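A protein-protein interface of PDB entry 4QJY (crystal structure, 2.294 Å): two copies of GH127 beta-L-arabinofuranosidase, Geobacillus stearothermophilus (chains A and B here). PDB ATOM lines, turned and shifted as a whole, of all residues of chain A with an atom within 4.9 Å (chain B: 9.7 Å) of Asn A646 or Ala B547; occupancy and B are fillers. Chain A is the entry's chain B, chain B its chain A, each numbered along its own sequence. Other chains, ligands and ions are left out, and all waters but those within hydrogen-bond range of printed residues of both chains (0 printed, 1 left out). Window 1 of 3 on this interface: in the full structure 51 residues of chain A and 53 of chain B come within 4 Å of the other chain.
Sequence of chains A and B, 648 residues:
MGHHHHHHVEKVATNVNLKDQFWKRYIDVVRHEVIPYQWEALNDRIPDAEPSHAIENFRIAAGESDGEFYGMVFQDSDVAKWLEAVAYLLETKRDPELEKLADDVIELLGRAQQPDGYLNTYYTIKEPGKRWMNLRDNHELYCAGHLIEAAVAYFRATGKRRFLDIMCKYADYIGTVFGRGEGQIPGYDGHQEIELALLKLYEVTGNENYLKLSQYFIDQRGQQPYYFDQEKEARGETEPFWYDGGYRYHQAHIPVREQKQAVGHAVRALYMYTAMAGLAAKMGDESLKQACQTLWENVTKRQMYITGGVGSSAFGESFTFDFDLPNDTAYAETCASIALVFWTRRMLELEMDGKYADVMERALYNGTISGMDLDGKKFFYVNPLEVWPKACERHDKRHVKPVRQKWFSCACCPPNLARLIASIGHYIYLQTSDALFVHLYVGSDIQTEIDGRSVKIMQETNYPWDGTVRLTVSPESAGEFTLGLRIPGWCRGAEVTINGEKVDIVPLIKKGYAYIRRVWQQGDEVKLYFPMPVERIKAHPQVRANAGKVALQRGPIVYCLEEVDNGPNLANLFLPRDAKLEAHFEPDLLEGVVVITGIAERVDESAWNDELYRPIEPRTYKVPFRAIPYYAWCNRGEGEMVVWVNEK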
ATOM      1  N   GLY A 548      20.638 -11.240 -13.781  1.00  0.00           N
ATOM      2  CA  GLY A 548      20.669  -9.801 -13.605  1.00  0.00           C
ATOM      3  C   GLY A 548      21.896  -9.083 -14.124  1.00  0.00           C
ATOM      4  O   GLY A 548      22.090  -7.892 -13.851  1.00  0.00           O
ATOM      5  N   LYS A 549      22.723  -9.816 -14.869  1.00  0.00           N
ATOM      6  CA  LYS A 549      23.972  -9.319 -15.395  1.00  0.00           C
ATOM      7  C   LYS A 549      24.010  -9.300 -16.919  1.00  0.00           C
ATOM      8  O   LYS A 549      23.327 -10.091 -17.565  1.00  0.00           O
ATOM      9  CB  LYS A 549      25.084 -10.220 -14.917  1.00  0.00           C
ATOM     10  CG  LYS A 549      25.379 -10.104 -13.438  1.00  0.00           C
ATOM     11  CD  LYS A 549      26.689 -10.801 -13.131  1.00  0.00           C
ATOM     12  CE  LYS A 549      26.801 -11.197 -11.679  1.00  0.00           C
ATOM     13  NZ  LYS A 549      26.988  -9.959 -10.917  1.00  0.00           N
ATOM     14  N   ALA A 571      31.445  -4.094  -8.796  1.00  0.00           N
ATOM     15  CA  ALA A 571      30.163  -4.771  -8.523  1.00  0.00           C
ATOM     16  C   ALA A 571      29.051  -3.733  -8.434  1.00  0.00           C
ATOM     17  O   ALA A 571      27.920  -4.011  -8.804  1.00  0.00           O
ATOM     18  CB  ALA A 571      30.238  -5.576  -7.240  1.00  0.00           C
ATOM     19  N   ASN A 572      29.402  -2.524  -7.990  1.00  0.00           N
ATOM     20  CA  ASN A 572      28.438  -1.434  -7.873  1.00  0.00           C
ATOM     21  C   ASN A 572      28.519  -0.384  -9.002  1.00  0.00           C
ATOM     22  O   ASN A 572      28.271   0.801  -8.790  1.00  0.00           O
ATOM     23  CB  ASN A 572      28.556  -0.803  -6.468  1.00  0.00           C
ATOM     24  CG  ASN A 572      27.928  -1.701  -5.389  1.00  0.00           C
ATOM     25  OD1 ASN A 572      26.735  -1.577  -5.065  1.00  0.00           O
ATOM     26  ND2 ASN A 572      28.693  -2.673  -4.915  1.00  0.00           N
ATOM     27  N   LEU A 573      28.878  -0.837 -10.208  1.00  0.00           N
ATOM     28  CA  LEU A 573      28.689  -0.070 -11.430  1.00  0.00           C
ATOM     29  C   LEU A 573      27.575  -0.736 -12.170  1.00  0.00           C
ATOM     30  O   LEU A 573      27.734  -1.875 -12.572  1.00  0.00           O
ATOM     31  CB  LEU A 573      29.924  -0.145 -12.314  1.00  0.00           C
ATOM     32  CG  LEU A 573      30.772   1.083 -12.474  1.00  0.00           C
ATOM     33  CD1 LEU A 573      31.873   0.791 -13.465  1.00  0.00           C
ATOM     34  CD2 LEU A 573      29.975   2.313 -12.886  1.00  0.00           C
ATOM     35  N   PHE A 574      26.472  -0.047 -12.384  1.00  0.00           N
ATOM     36  CA  PHE A 574      25.321  -0.636 -13.063  1.00  0.00           C
ATOM     37  C   PHE A 574      25.175  -0.098 -14.477  1.00  0.00           C
ATOM     38  O   PHE A 574      25.335   1.075 -14.693  1.00  0.00           O
ATOM     39  CB  PHE A 574      24.032  -0.371 -12.273  1.00  0.00           C
ATOM     40  CG  PHE A 574      23.976  -1.133 -10.998  1.00  0.00           C
ATOM     41  CD1 PHE A 574      24.723  -0.730  -9.918  1.00  0.00           C
ATOM     42  CD2 PHE A 574      23.244  -2.306 -10.915  1.00  0.00           C
ATOM     43  CE1 PHE A 574      24.735  -1.447  -8.766  1.00  0.00           C
ATOM     44  CE2 PHE A 574      23.247  -3.032  -9.733  1.00  0.00           C
ATOM     45  CZ  PHE A 574      24.002  -2.610  -8.682  1.00  0.00           C
ATOM     46  N   LEU A 575      24.826  -0.956 -15.424  1.00  0.00           N
ATOM     47  CA  LEU A 575      24.651  -0.541 -16.800  1.00  0.00           C
ATOM     48  C   LEU A 575      23.162  -0.524 -17.095  1.00  0.00           C
ATOM     49  O   LEU A 575      22.550  -1.588 -17.165  1.00  0.00           O
ATOM     50  CB  LEU A 575      25.358  -1.492 -17.746  1.00  0.00           C
ATOM     51  CG  LEU A 575      25.380  -0.940 -19.179  1.00  0.00           C
ATOM     52  CD1 LEU A 575      26.450   0.139 -19.281  1.00  0.00           C
ATOM     53  CD2 LEU A 575      25.617  -2.029 -20.230  1.00  0.00           C
ATOM     54  N   TRP A 644      30.946  -9.692 -16.447  1.00  0.00           N
ATOM     55  CA  TRP A 644      29.525  -9.687 -16.354  1.00  0.00           C
ATOM     56  C   TRP A 644      29.171  -8.541 -15.452  1.00  0.00           C
ATOM     57  O   TRP A 644      29.599  -8.497 -14.345  1.00  0.00           O
ATOM     58  CB  TRP A 644      29.049 -11.025 -15.856  1.00  0.00           C
ATOM     59  CG  TRP A 644      29.125 -12.018 -16.893  1.00  0.00           C
ATOM     60  CD1 TRP A 644      30.116 -12.930 -17.078  1.00  0.00           C
ATOM     61  CD2 TRP A 644      28.167 -12.248 -17.936  1.00  0.00           C
ATOM     62  NE1 TRP A 644      29.822 -13.735 -18.148  1.00  0.00           N
ATOM     63  CE2 TRP A 644      28.627 -13.331 -18.690  1.00  0.00           C
ATOM     64  CE3 TRP A 644      26.934 -11.673 -18.276  1.00  0.00           C
ATOM     65  CZ2 TRP A 644      27.912 -13.823 -19.802  1.00  0.00           C
ATOM     66  CZ3 TRP A 644      26.236 -12.179 -19.337  1.00  0.00           C
ATOM     67  CH2 TRP A 644      26.726 -13.220 -20.104  1.00  0.00           C
ATOM     68  N   VAL A 645      28.462  -7.556 -15.972  1.00  0.00           N
ATOM     69  CA  VAL A 645      28.160  -6.395 -15.179  1.00  0.00           C
ATOM     70  C   VAL A 645      26.722  -6.356 -14.769  1.00  0.00           C
ATOM     71  O   VAL A 645      25.838  -6.823 -15.491  1.00  0.00           O
ATOM     72  CB  VAL A 645      28.807  -5.076 -15.734  1.00  0.00           C
ATOM     73  CG1 VAL A 645      29.776  -5.339 -16.864  1.00  0.00           C
ATOM     74  CG2 VAL A 645      27.818  -3.975 -16.017  1.00  0.00           C
ATOM     75  N   ASN A 646      26.480  -5.821 -13.596  1.00  0.00           N
ATOM     76  CA  ASN A 646      25.129  -5.692 -13.118  1.00  0.00           C
ATOM     77  C   ASN A 646      24.296  -4.770 -13.941  1.00  0.00           C
ATOM     78  O   ASN A 646      24.710  -3.717 -14.279  1.00  0.00           O
ATOM     79  CB  ASN A 646      25.096  -5.288 -11.653  1.00  0.00           C
ATOM     80  CG  ASN A 646      25.544  -6.381 -10.763  1.00  0.00           C
ATOM     81  OD1 ASN A 646      26.420  -6.205  -9.983  1.00  0.00           O
ATOM     82  ND2 ASN A 646      24.943  -7.513 -10.884  1.00  0.00           N
ATOM     83  N   GLU A 647      23.102  -5.214 -14.247  1.00  0.00           N
ATOM     84  CA  GLU A 647      22.180  -4.481 -15.079  1.00  0.00           C
ATOM     85  C   GLU A 647      21.208  -3.581 -14.321  1.00  0.00           C
ATOM     86  O   GLU A 647      20.784  -3.888 -13.258  1.00  0.00           O
ATOM     87  CB  GLU A 647      21.443  -5.412 -16.017  1.00  0.00           C
ATOM     88  CG  GLU A 647      20.944  -4.723 -17.251  1.00  0.00           C
ATOM     89  CD  GLU A 647      20.562  -5.651 -18.371  1.00  0.00           C
ATOM     90  OE1 GLU A 647      19.789  -6.577 -18.136  1.00  0.00           O
ATOM     91  OE2 GLU A 647      21.001  -5.431 -19.499  1.00  0.00           O
ATOM     92  N   LYS A 648      20.908  -2.455 -14.940  1.00  0.00           N
ATOM     93  CA  LYS A 648      20.042  -1.379 -14.477  1.00  0.00           C
ATOM     94  C   LYS A 648      20.125  -0.975 -13.044  1.00  0.00           C
ATOM     95  O   LYS A 648      20.150   0.197 -12.771  1.00  0.00           O
ATOM     96  CB  LYS A 648      18.594  -1.598 -14.862  1.00  0.00           C
ATOM     97  CG  LYS A 648      18.271  -1.144 -16.266  1.00  0.00           C
ATOM     98  CD  LYS A 648      17.049  -0.263 -16.299  1.00  0.00           C
ATOM     99  CE  LYS A 648      16.849   0.332 -17.684  1.00  0.00           C
ATOM    100  NZ  LYS A 648      17.193   1.765 -17.826  1.00  0.00           N
ATOM    101  N   PHE B 323      34.071  -6.671   4.329  1.00  0.00           N
ATOM    102  CA  PHE B 323      33.056  -6.654   3.299  1.00  0.00           C
ATOM    103  C   PHE B 323      33.047  -7.866   2.386  1.00  0.00           C
ATOM    104  O   PHE B 323      32.310  -7.857   1.449  1.00  0.00           O
ATOM    105  CB  PHE B 323      33.138  -5.381   2.491  1.00  0.00           C
ATOM    106  CG  PHE B 323      32.994  -4.124   3.314  1.00  0.00           C
ATOM    107  CD1 PHE B 323      31.790  -3.818   3.957  1.00  0.00           C
ATOM    108  CD2 PHE B 323      34.013  -3.188   3.354  1.00  0.00           C
ATOM    109  CE1 PHE B 323      31.619  -2.622   4.660  1.00  0.00           C
ATOM    110  CE2 PHE B 323      33.858  -1.995   4.067  1.00  0.00           C
ATOM    111  CZ  PHE B 323      32.645  -1.713   4.714  1.00  0.00           C
ATOM    112  N   LEU B 325      31.683 -11.144   2.064  1.00  0.00           N
ATOM    113  CA  LEU B 325      30.576 -11.874   2.660  1.00  0.00           C
ATOM    114  C   LEU B 325      29.785 -12.642   1.610  1.00  0.00           C
ATOM    115  O   LEU B 325      28.589 -12.392   1.389  1.00  0.00           O
ATOM    116  CB  LEU B 325      29.676 -10.915   3.427  1.00  0.00           C
ATOM    117  CG  LEU B 325      30.286 -10.230   4.639  1.00  0.00           C
ATOM    118  CD1 LEU B 325      29.527  -8.956   5.000  1.00  0.00           C
ATOM    119  CD2 LEU B 325      30.266 -11.162   5.816  1.00  0.00           C
ATOM    120  N   ASN B 327      27.580 -15.513  -0.118  1.00  0.00           N
ATOM    121  CA  ASN B 327      26.421 -16.182   0.429  1.00  0.00           C
ATOM    122  C   ASN B 327      26.442 -17.661   0.224  1.00  0.00           C
ATOM    123  O   ASN B 327      25.948 -18.409   1.055  1.00  0.00           O
ATOM    124  CB  ASN B 327      25.146 -15.556  -0.163  1.00  0.00           C
ATOM    125  CG  ASN B 327      24.980 -14.111   0.289  1.00  0.00           C
ATOM    126  OD1 ASN B 327      25.014 -13.828   1.476  1.00  0.00           O
ATOM    127  ND2 ASN B 327      24.782 -13.210  -0.641  1.00  0.00           N
ATOM    128  N   ILE B 537      15.871  -4.813   2.890  1.00  0.00           N
ATOM    129  CA  ILE B 537      17.162  -4.511   3.474  1.00  0.00           C
ATOM    130  C   ILE B 537      18.228  -4.509   2.355  1.00  0.00           C
ATOM    131  O   ILE B 537      18.274  -5.406   1.504  1.00  0.00           O
ATOM    132  CB  ILE B 537      17.473  -5.509   4.620  1.00  0.00           C
ATOM    133  CG1 ILE B 537      16.347  -5.483   5.666  1.00  0.00           C
ATOM    134  CG2 ILE B 537      18.796  -5.156   5.274  1.00  0.00           C
ATOM    135  CD1 ILE B 537      16.271  -4.144   6.378  1.00  0.00           C
ATOM    136  N   LYS B 538      19.040  -3.461   2.352  1.00  0.00           N
ATOM    137  CA  LYS B 538      20.209  -3.347   1.512  1.00  0.00           C
ATOM    138  C   LYS B 538      21.496  -3.496   2.303  1.00  0.00           C
ATOM    139  O   LYS B 538      21.602  -3.044   3.443  1.00  0.00           O
ATOM    140  CB  LYS B 538      20.250  -2.002   0.802  1.00  0.00           C
ATOM    141  CG  LYS B 538      19.086  -1.768  -0.133  1.00  0.00           C
ATOM    142  CD  LYS B 538      18.989  -2.689  -1.343  1.00  0.00           C
ATOM    143  CE  LYS B 538      20.091  -2.389  -2.346  1.00  0.00           C
ATOM    144  NZ  LYS B 538      20.186  -3.444  -3.392  1.00  0.00           N
ATOM    145  N   ALA B 539      22.492  -4.117   1.674  1.00  0.00           N
ATOM    146  CA  ALA B 539      23.814  -4.123   2.243  1.00  0.00           C
ATOM    147  C   ALA B 539      24.603  -2.895   1.789  1.00  0.00           C
ATOM    148  O   ALA B 539      24.395  -2.332   0.688  1.00  0.00           O
ATOM    149  CB  ALA B 539      24.536  -5.373   1.823  1.00  0.00           C
ATOM    150  N   HIS B 540      25.552  -2.521   2.615  1.00  0.00           N
ATOM    151  CA  HIS B 540      26.461  -1.497   2.289  1.00  0.00           C
ATOM    152  C   HIS B 540      27.051  -1.819   0.897  1.00  0.00           C
ATOM    153  O   HIS B 540      27.332  -2.945   0.608  1.00  0.00           O
ATOM    154  CB  HIS B 540      27.558  -1.441   3.341  1.00  0.00           C
ATOM    155  CG  HIS B 540      28.428  -0.238   3.233  1.00  0.00           C
ATOM    156  ND1 HIS B 540      29.330  -0.071   2.214  1.00  0.00           N
ATOM    157  CD2 HIS B 540      28.556   0.845   4.033  1.00  0.00           C
ATOM    158  CE1 HIS B 540      29.985   1.060   2.389  1.00  0.00           C
ATOM    159  NE2 HIS B 540      29.533   1.625   3.497  1.00  0.00           N
ATOM    160  N   PRO B 541      27.246  -0.804   0.051  1.00  0.00           N
ATOM    161  CA  PRO B 541      27.755  -0.995  -1.313  1.00  0.00           C
ATOM    162  C   PRO B 541      29.099  -1.750  -1.409  1.00  0.00           C
ATOM    163  O   PRO B 541      29.310  -2.492  -2.381  1.00  0.00           O
ATOM    164  CB  PRO B 541      27.906   0.444  -1.833  1.00  0.00           C
ATOM    165  CG  PRO B 541      26.838   1.188  -1.081  1.00  0.00           C
ATOM    166  CD  PRO B 541      26.843   0.598   0.299  1.00  0.00           C
ATOM    167  N   GLN B 542      29.988  -1.586  -0.427  1.00  0.00           N
ATOM    168  CA  GLN B 542      31.232  -2.373  -0.390  1.00  0.00           C
ATOM    169  C   GLN B 542      31.034  -3.896  -0.306  1.00  0.00           C
ATOM    170  O   GLN B 542      31.975  -4.627  -0.581  1.00  0.00           O
ATOM    171  CB  GLN B 542      32.130  -1.946   0.739  1.00  0.00           C
ATOM    172  CG  GLN B 542      32.677  -0.540   0.628  1.00  0.00           C
ATOM    173  CD  GLN B 542      33.734  -0.451  -0.437  1.00  0.00           C
ATOM    174  OE1 GLN B 542      34.647  -1.264  -0.492  1.00  0.00           O
ATOM    175  NE2 GLN B 542      33.571   0.470  -1.323  1.00  0.00           N
ATOM    176  N   VAL B 543      29.844  -4.374   0.079  1.00  0.00           N
ATOM    177  CA  VAL B 543      29.580  -5.817   0.097  1.00  0.00           C
ATOM    178  C   VAL B 543      29.240  -6.213  -1.289  1.00  0.00           C
ATOM    179  O   VAL B 543      28.101  -6.078  -1.745  1.00  0.00           O
ATOM    180  CB  VAL B 543      28.445  -6.241   1.019  1.00  0.00           C
ATOM    181  CG1 VAL B 543      28.318  -7.754   0.962  1.00  0.00           C
ATOM    182  CG2 VAL B 543      28.729  -5.754   2.469  1.00  0.00           C
ATOM    183  N   ARG B 544      30.269  -6.649  -1.975  1.00  0.00           N
ATOM    184  CA  ARG B 544      30.178  -7.006  -3.367  1.00  0.00           C
ATOM    185  C   ARG B 544      29.116  -8.025  -3.654  1.00  0.00           C
ATOM    186  O   ARG B 544      28.333  -7.877  -4.575  1.00  0.00           O
ATOM    187  CB  ARG B 544      31.500  -7.604  -3.768  1.00  0.00           C
ATOM    188  CG  ARG B 544      32.446  -6.621  -4.387  1.00  0.00           C
ATOM    189  CD  ARG B 544      32.897  -5.583  -3.458  1.00  0.00           C
ATOM    190  NE  ARG B 544      34.004  -4.859  -4.076  1.00  0.00           N
ATOM    191  CZ  ARG B 544      34.675  -3.892  -3.461  1.00  0.00           C
ATOM    192  NH1 ARG B 544      34.352  -3.506  -2.226  1.00  0.00           N
ATOM    193  NH2 ARG B 544      35.676  -3.307  -4.085  1.00  0.00           N
ATOM    194  N   ALA B 545      29.098  -9.050  -2.835  1.00  0.00           N
ATOM    195  CA  ALA B 545      28.215 -10.162  -2.988  1.00  0.00           C
ATOM    196  C   ALA B 545      26.761  -9.752  -3.180  1.00  0.00           C
ATOM    197  O   ALA B 545      26.014 -10.469  -3.832  1.00  0.00           O
ATOM    198  CB  ALA B 545      28.342 -11.083  -1.762  1.00  0.00           C
ATOM    199  N   ASN B 546      26.363  -8.629  -2.590  1.00  0.00           N
ATOM    200  CA  ASN B 546      24.953  -8.247  -2.555  1.00  0.00           C
ATOM    201  C   ASN B 546      24.575  -7.003  -3.415  1.00  0.00           C
ATOM    202  O   ASN B 546      23.423  -6.521  -3.368  1.00  0.00           O
ATOM    203  CB  ASN B 546      24.547  -8.081  -1.086  1.00  0.00           C
ATOM    204  CG  ASN B 546      24.641  -9.384  -0.315  1.00  0.00           C
ATOM    205  OD1 ASN B 546      24.303 -10.425  -0.829  1.00  0.00           O
ATOM    206  ND2 ASN B 546      25.066  -9.313   0.928  1.00  0.00           N
ATOM    207  N   ALA B 547      25.541  -6.500  -4.192  1.00  0.00           N
ATOM    208  CA  ALA B 547      25.253  -5.519  -5.234  1.00  0.00           C
ATOM    209  C   ALA B 547      24.047  -6.005  -6.019  1.00  0.00           C
ATOM    210  O   ALA B 547      24.008  -7.134  -6.472  1.00  0.00           O
ATOM    211  CB  ALA B 547      26.485  -5.315  -6.168  1.00  0.00           C
ATOM    212  N   GLY B 548      23.049  -5.158  -6.201  1.00  0.00           N
ATOM    213  CA  GLY B 548      21.868  -5.572  -6.965  1.00  0.00           C
ATOM    214  C   GLY B 548      20.938  -6.595  -6.320  1.00  0.00           C
ATOM    215  O   GLY B 548      20.053  -7.140  -6.992  1.00  0.00           O
ATOM    216  N   LYS B 549      21.085  -6.831  -5.027  1.00  0.00           N
ATOM    217  CA  LYS B 549      20.222  -7.818  -4.316  1.00  0.00           C
ATOM    218  C   LYS B 549      19.563  -7.175  -3.120  1.00  0.00           C
ATOM    219  O   LYS B 549      20.055  -6.159  -2.606  1.00  0.00           O
ATOM    220  CB  LYS B 549      21.065  -8.988  -3.815  1.00  0.00           C
ATOM    221  CG  LYS B 549      21.826  -9.766  -4.899  1.00  0.00           C
ATOM    222  CD  LYS B 549      22.548 -10.998  -4.336  1.00  0.00           C
ATOM    223  CE  LYS B 549      23.402 -11.726  -5.374  1.00  0.00           C
ATOM    224  NZ  LYS B 549      22.665 -12.034  -6.628  1.00  0.00           N
ATOM    225  N   VAL B 550      18.520  -7.806  -2.600  1.00  0.00           N
ATOM    226  CA  VAL B 550      17.793  -7.242  -1.474  1.00  0.00           C
ATOM    227  C   VAL B 550      17.291  -8.385  -0.613  1.00  0.00           C
ATOM    228  O   VAL B 550      17.024  -9.458  -1.110  1.00  0.00           O
ATOM    229  CB  VAL B 550      16.596  -6.396  -1.994  1.00  0.00           C
ATOM    230  CG1 VAL B 550      15.603  -7.260  -2.733  1.00  0.00           C
ATOM    231  CG2 VAL B 550      15.873  -5.664  -0.875  1.00  0.00           C
ATOM    232  N   PHE B 574      13.218 -12.015  -9.618  1.00  0.00           N
ATOM    233  CA  PHE B 574      13.561 -10.648  -9.489  1.00  0.00           C
ATOM    234  C   PHE B 574      12.407  -9.966  -8.790  1.00  0.00           C
ATOM    235  O   PHE B 574      11.213 -10.252  -9.056  1.00  0.00           O
ATOM    236  CB  PHE B 574      13.818 -10.057 -10.851  1.00  0.00           C
ATOM    237  CG  PHE B 574      14.943 -10.741 -11.586  1.00  0.00           C
ATOM    238  CD1 PHE B 574      14.698 -11.888 -12.332  1.00  0.00           C
ATOM    239  CD2 PHE B 574      16.238 -10.222 -11.530  1.00  0.00           C
ATOM    240  CE1 PHE B 574      15.731 -12.515 -12.987  1.00  0.00           C
ATOM    241  CE2 PHE B 574      17.276 -10.854 -12.175  1.00  0.00           C
ATOM    242  CZ  PHE B 574      17.018 -12.007 -12.895  1.00  0.00           C
ATOM    243  N   TRP B 644      19.441 -13.302  -0.038  1.00  0.00           N
ATOM    244  CA  TRP B 644      19.592 -12.094  -0.848  1.00  0.00           C
ATOM    245  C   TRP B 644      19.011 -12.314  -2.263  1.00  0.00           C
ATOM    246  O   TRP B 644      19.546 -13.094  -3.030  1.00  0.00           O
ATOM    247  CB  TRP B 644      21.032 -11.687  -0.931  1.00  0.00           C
ATOM    248  CG  TRP B 644      21.532 -11.157   0.371  1.00  0.00           C
ATOM    249  CD1 TRP B 644      22.185 -11.867   1.360  1.00  0.00           C
ATOM    250  CD2 TRP B 644      21.379  -9.846   0.860  1.00  0.00           C
ATOM    251  NE1 TRP B 644      22.420 -11.067   2.424  1.00  0.00           N
ATOM    252  CE2 TRP B 644      21.939  -9.816   2.149  1.00  0.00           C
ATOM    253  CE3 TRP B 644      20.842  -8.667   0.334  1.00  0.00           C
ATOM    254  CZ2 TRP B 644      22.018  -8.661   2.884  1.00  0.00           C
ATOM    255  CZ3 TRP B 644      20.896  -7.517   1.110  1.00  0.00           C
ATOM    256  CH2 TRP B 644      21.423  -7.539   2.378  1.00  0.00           C
ATOM    257  N   VAL B 645      17.902 -11.651  -2.596  1.00  0.00           N
ATOM    258  CA  VAL B 645      17.281 -11.865  -3.896  1.00  0.00           C
ATOM    259  C   VAL B 645      17.597 -10.751  -4.881  1.00  0.00           C
ATOM    260  O   VAL B 645      17.808  -9.597  -4.493  1.00  0.00           O
ATOM    261  CB  VAL B 645      15.777 -12.225  -3.776  1.00  0.00           C
ATOM    262  CG1 VAL B 645      15.244 -12.182  -2.341  1.00  0.00           C
ATOM    263  CG2 VAL B 645      14.909 -11.461  -4.722  1.00  0.00           C
ATOM    264  N   ASN B 646      17.651 -11.114  -6.137  1.00  0.00           N
ATOM    265  CA  ASN B 646      17.882 -10.150  -7.155  1.00  0.00           C
ATOM    266  C   ASN B 646      16.766  -9.135  -7.229  1.00  0.00           C
ATOM    267  O   ASN B 646      15.625  -9.448  -7.153  1.00  0.00           O
ATOM    268  CB  ASN B 646      18.126 -10.806  -8.496  1.00  0.00           C
ATOM    269  CG  ASN B 646      19.428 -11.531  -8.553  1.00  0.00           C
ATOM    270  OD1 ASN B 646      19.475 -12.671  -8.905  1.00  0.00           O
ATOM    271  ND2 ASN B 646      20.466 -10.876  -8.181  1.00  0.00           N
ATOM    272  N   GLU B 647      17.159  -7.899  -7.362  1.00  0.00           N
ATOM    273  CA  GLU B 647      16.255  -6.815  -7.536  1.00  0.00           C
ATOM    274  C   GLU B 647      16.044  -6.594  -8.989  1.00  0.00           C
ATOM    275  O   GLU B 647      16.935  -6.785  -9.751  1.00  0.00           O
ATOM    276  CB  GLU B 647      16.938  -5.591  -7.063  1.00  0.00           C
ATOM    277  CG  GLU B 647      16.391  -4.910  -5.858  1.00  0.00           C
ATOM    278  CD  GLU B 647      17.370  -3.885  -5.325  1.00  0.00           C
ATOM    279  OE1 GLU B 647      18.466  -3.694  -5.898  1.00  0.00           O
ATOM    280  OE2 GLU B 647      17.042  -3.263  -4.336  1.00  0.00           O
ATOM    281  N   LYS B 648      14.869  -6.171  -9.379  1.00  0.00           N
ATOM    282  CA  LYS B 648      14.684  -5.653 -10.708  1.00  0.00           C
ATOM    283  C   LYS B 648      14.826  -4.159 -10.622  1.00  0.00           C
ATOM    284  O   LYS B 648      15.775  -3.588 -11.152  1.00  0.00           O
ATOM    285  CB  LYS B 648      13.336  -6.022 -11.272  1.00  0.00           C
ATOM    286  CG  LYS B 648      13.190  -5.580 -12.705  1.00  0.00           C
ATOM    287  CD  LYS B 648      11.770  -5.679 -13.213  1.00  0.00           C
ATOM    288  CE  LYS B 648      11.733  -6.512 -14.478  1.00  0.00           C
ATOM    289  NZ  LYS B 648      10.784  -6.009 -15.501  1.00  0.00           N
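O of Pro B541 sits at hydrogen-bond distance from ND2 of Asn A572, 2.6 Å away.
OE1 of Gln B542 sits at hydrogen-bond distance from NH1 of Arg B544 (2.8 Å).
The backbone carbonyl oxygen (O) of Gly B548 is in hydrogen-bond range of the backbone NH (N) of Glu B647 (3.0 Å).
The backbone carbonyl oxygen (O) of Gly A548 sits at hydrogen-bond distance from the backbone NH (N) of Glu A647, 2.9 Å away.
The side-chain amino group of Lys A549 lies close to the side-chain amide nitrogen of Asn A646 (3.2 Å).
The backbone carbonyl oxygen (O) of Ala A571 lies close to the side-chain amide oxygen (OD1) of Asn A646 (2.9 Å).
The backbone NH (N) of Leu A575 sits at hydrogen-bond distance from the backbone carbonyl oxygen (O) of Asn A646 (3.0 Å).
Among the printed residues, merely in contact across the chains: Gly A548 with Phe B574 (3.7 Å), Ala A571 with Arg B544 (3.8 Å), Ala A571 with Ala B547 (3.3 Å), Asn A572 with Ala B547 (3.7 Å), Phe A574 with Gly B548 (3.7 Å) and Asn A646 with Ala B547 (3.9 Å).
Ala A571 touches two residues of chain B.
Printed residues of chain B within 4 Å of Asn A572: Pro B541 and Ala B547.
No residue of chain B comes within 4 Å of Val A645.
Asn A646 touches one residue of chain B.
Phe B323 touches none of the printed residues of chain A.
Of chain A, only Ala A571, Asn A572 and Asn A646 come within 4 Å of Ala B547.
Of the printed residues of chain A, Gly B548 touches Phe A574 (3.7 Å).
The nearest residue of chain B that does not touch Asn A646 is Gly B548 (5.2 Å).
Of the 23 printed residues of chain B, 5 touch a printed residue of chain A.
Printed residues of chain B that touch a printed residue of chain A: Pro B541, Arg B544, Ala B547, Gly B548 and Phe B574.
Hydrophobic or aromatic side chains of chain B that line the printed part of chain A: Pro B541, Ala B547 and Phe B574.
Of the 12 printed residues of chain A, 5 touch a printed residue of chain B.
Among the printed residues, no Asp or Glu carboxylate lies within 4 Å of a Lys or Arg side-chain nitrogen of the other chain.
Gly A548 touches Phe B574, and with the chains exchanged Phe A574 touches Gly B548.
8 positions are printed for both chains.
Of the 7 pairs that touch across the chains among the printed residues, 2 have their exchanged pair printed and touching as well.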
